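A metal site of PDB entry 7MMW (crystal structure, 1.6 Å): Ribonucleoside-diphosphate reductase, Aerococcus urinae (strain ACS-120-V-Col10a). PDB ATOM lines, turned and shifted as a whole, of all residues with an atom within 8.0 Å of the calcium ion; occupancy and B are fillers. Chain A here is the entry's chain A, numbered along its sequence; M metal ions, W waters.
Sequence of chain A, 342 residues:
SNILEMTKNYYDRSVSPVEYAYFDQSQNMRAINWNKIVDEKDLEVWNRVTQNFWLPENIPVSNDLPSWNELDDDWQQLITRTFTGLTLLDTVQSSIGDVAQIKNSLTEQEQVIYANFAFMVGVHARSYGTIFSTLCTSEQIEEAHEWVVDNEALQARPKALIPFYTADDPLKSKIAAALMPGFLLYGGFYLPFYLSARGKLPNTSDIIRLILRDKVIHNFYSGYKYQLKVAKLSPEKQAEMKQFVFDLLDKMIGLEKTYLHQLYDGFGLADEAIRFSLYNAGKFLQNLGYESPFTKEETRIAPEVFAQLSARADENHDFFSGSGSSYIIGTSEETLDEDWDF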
ATOM      1  N   TYR A 190       5.880  27.585 -19.976  1.00  0.00           N
ATOM      2  CA  TYR A 190       4.738  26.632 -20.051  1.00  0.00           C
ATOM      3  C   TYR A 190       4.927  25.520 -19.018  1.00  0.00           C
ATOM      4  O   TYR A 190       3.947  25.162 -18.339  1.00  0.00           O
ATOM      5  CB  TYR A 190       4.595  26.031 -21.447  1.00  0.00           C
ATOM      6  CG  TYR A 190       3.558  24.937 -21.489  1.00  0.00           C
ATOM      7  CD1 TYR A 190       2.210  25.239 -21.499  1.00  0.00           C
ATOM      8  CD2 TYR A 190       3.940  23.610 -21.438  1.00  0.00           C
ATOM      9  CE1 TYR A 190       1.246  24.234 -21.488  1.00  0.00           C
ATOM     10  CE2 TYR A 190       2.997  22.597 -21.427  1.00  0.00           C
ATOM     11  CZ  TYR A 190       1.649  22.913 -21.446  1.00  0.00           C
ATOM     12  OH  TYR A 190       0.725  21.901 -21.425  1.00  0.00           O
ATOM     13  N   PHE A 267       7.537  13.538 -23.814  1.00  0.00           N
ATOM     14  CA  PHE A 267       6.525  14.106 -22.888  1.00  0.00           C
ATOM     15  C   PHE A 267       5.246  14.494 -23.638  1.00  0.00           C
ATOM     16  O   PHE A 267       4.219  14.673 -22.973  1.00  0.00           O
ATOM     17  CB  PHE A 267       7.100  15.307 -22.138  1.00  0.00           C
ATOM     18  CG  PHE A 267       8.242  14.970 -21.217  1.00  0.00           C
ATOM     19  CD1 PHE A 267       8.005  14.608 -19.895  1.00  0.00           C
ATOM     20  CD2 PHE A 267       9.552  14.990 -21.659  1.00  0.00           C
ATOM     21  CE1 PHE A 267       9.051  14.299 -19.051  1.00  0.00           C
ATOM     22  CE2 PHE A 267      10.596  14.672 -20.818  1.00  0.00           C
ATOM     23  CZ  PHE A 267      10.342  14.319 -19.504  1.00  0.00           C
ATOM     24  N   GLY A 268       5.313  14.654 -24.966  1.00  0.00           N
ATOM     25  CA  GLY A 268       4.154  15.046 -25.797  1.00  0.00           C
ATOM     26  C   GLY A 268       3.638  16.449 -25.488  1.00  0.00           C
ATOM     27  O   GLY A 268       2.480  16.723 -25.866  1.00  0.00           O
ATOM     28  N   LEU A 269       4.438  17.312 -24.854  1.00  0.00           N
ATOM     29  CA  LEU A 269       4.006  18.667 -24.396  1.00  0.00           C
ATOM     30  C   LEU A 269       4.365  19.749 -25.427  1.00  0.00           C
ATOM     31  O   LEU A 269       3.955  20.904 -25.199  1.00  0.00           O
ATOM     32  CB  LEU A 269       4.657  18.980 -23.049  1.00  0.00           C
ATOM     33  CG  LEU A 269       4.176  18.162 -21.863  1.00  0.00           C
ATOM     34  CD1 LEU A 269       4.954  18.524 -20.611  1.00  0.00           C
ATOM     35  CD2 LEU A 269       2.686  18.347 -21.631  1.00  0.00           C
ATOM     36  N   ALA A 270       5.101  19.420 -26.487  1.00  0.00           N
ATOM     37  CA  ALA A 270       5.592  20.408 -27.487  1.00  0.00           C
ATOM     38  C   ALA A 270       4.413  21.197 -28.075  1.00  0.00           C
ATOM     39  O   ALA A 270       4.508  22.432 -28.126  1.00  0.00           O
ATOM     40  CB  ALA A 270       6.399  19.720 -28.558  1.00  0.00           C
ATOM     41  N   ASP A 271       3.343  20.522 -28.497  1.00  0.00           N
ATOM     42  CA  ASP A 271       2.196  21.194 -29.174  1.00  0.00           C
ATOM     43  C   ASP A 271       1.535  22.186 -28.204  1.00  0.00           C
ATOM     44  O   ASP A 271       1.240  23.315 -28.634  1.00  0.00           O
ATOM     45  CB  ASP A 271       1.212  20.197 -29.767  1.00  0.00           C
ATOM     46  CG  ASP A 271       0.811  19.078 -28.812  1.00  0.00           C
ATOM     47  OD1 ASP A 271       1.717  18.332 -28.378  1.00  0.00           O
ATOM     48  OD2 ASP A 271      -0.394  18.977 -28.515  1.00  0.00           O
ATOM     49  N   GLU A 272       1.336  21.803 -26.931  1.00  0.00           N
ATOM     50  CA  GLU A 272       0.744  22.695 -25.910  1.00  0.00           C
ATOM     51  C   GLU A 272       1.670  23.898 -25.664  1.00  0.00           C
ATOM     52  O   GLU A 272       1.177  25.039 -25.603  1.00  0.00           O
ATOM     53  CB  GLU A 272       0.495  21.946 -24.591  1.00  0.00           C
ATOM     54  CG  GLU A 272      -0.624  20.926 -24.661  1.00  0.00           C
ATOM     55  CD  GLU A 272      -0.277  19.594 -25.294  1.00  0.00           C
ATOM     56  OE1 GLU A 272       0.914  19.380 -25.635  1.00  0.00           O
ATOM     57  OE2 GLU A 272      -1.192  18.763 -25.456  1.00  0.00           O
ATOM     58  N   ALA A 273       2.974  23.637 -25.525  1.00  0.00           N
ATOM     59  CA  ALA A 273       3.990  24.682 -25.280  1.00  0.00           C
ATOM     60  C   ALA A 273       4.016  25.659 -26.459  1.00  0.00           C
ATOM     61  O   ALA A 273       4.133  26.883 -26.230  1.00  0.00           O
ATOM     62  CB  ALA A 273       5.344  24.057 -25.047  1.00  0.00           C
ATOM     63  N   ARG A 275       1.512  26.346 -28.659  1.00  0.00           N
ATOM     64  CA  ARG A 275       0.272  27.168 -28.640  1.00  0.00           C
ATOM     65  C   ARG A 275       0.437  28.298 -27.614  1.00  0.00           C
ATOM     66  O   ARG A 275       0.059  29.439 -27.917  1.00  0.00           O
ATOM     67  CB  ARG A 275      -0.962  26.322 -28.328  1.00  0.00           C
ATOM     68  CG  ARG A 275      -1.323  25.336 -29.428  1.00  0.00           C
ATOM     69  CD  ARG A 275      -2.769  24.901 -29.333  1.00  0.00           C
ATOM     70  NE  ARG A 275      -3.086  24.204 -28.095  1.00  0.00           N
ATOM     71  CZ  ARG A 275      -2.904  22.898 -27.879  1.00  0.00           C
ATOM     72  NH1 ARG A 275      -2.367  22.122 -28.815  1.00  0.00           N
ATOM     73  NH2 ARG A 275      -3.247  22.373 -26.719  1.00  0.00           N
HETATM   74 CA    CA M   1       0.380  17.180 -26.728  1.00  0.00          CA
HETATM   75  O   HOH W   1       0.938  15.346 -28.248  1.00  0.00           O
HETATM   76  O   HOH W   2      -1.722  16.624 -27.576  1.00  0.00           O
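The side-chain carboxylate (OD2) of Asp 271 lies close to the guanidinium group (NH1) of Arg 275 (3.7 Å).
The calcium ion is bound by the backbone carbonyl oxygen (O) of Gly 268 (2.3 Å). Water W2 binds the calcium ion (2.3 Å). The calcium ion is bound by OD1 of Asp 271 (2.4 Å). Water W1 is bound to the calcium ion (2.4 Å). OE1 of Glu 272 binds the calcium ion (2.5 Å). OE2 of Glu 272 is bound to the calcium ion (2.6 Å). OD2 of Asp 271 is bound to the calcium ion. The calcium ion has seven donor atoms within binding distance.
Of the 9 residues printed, 3 come within 4 Å of the calcium ion. Along chain A the residues within 4 Å of the calcium ion span positions 268 to 272. The nearest printed residue that does not touch the calcium ion is Leu 269 (4.5 Å).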
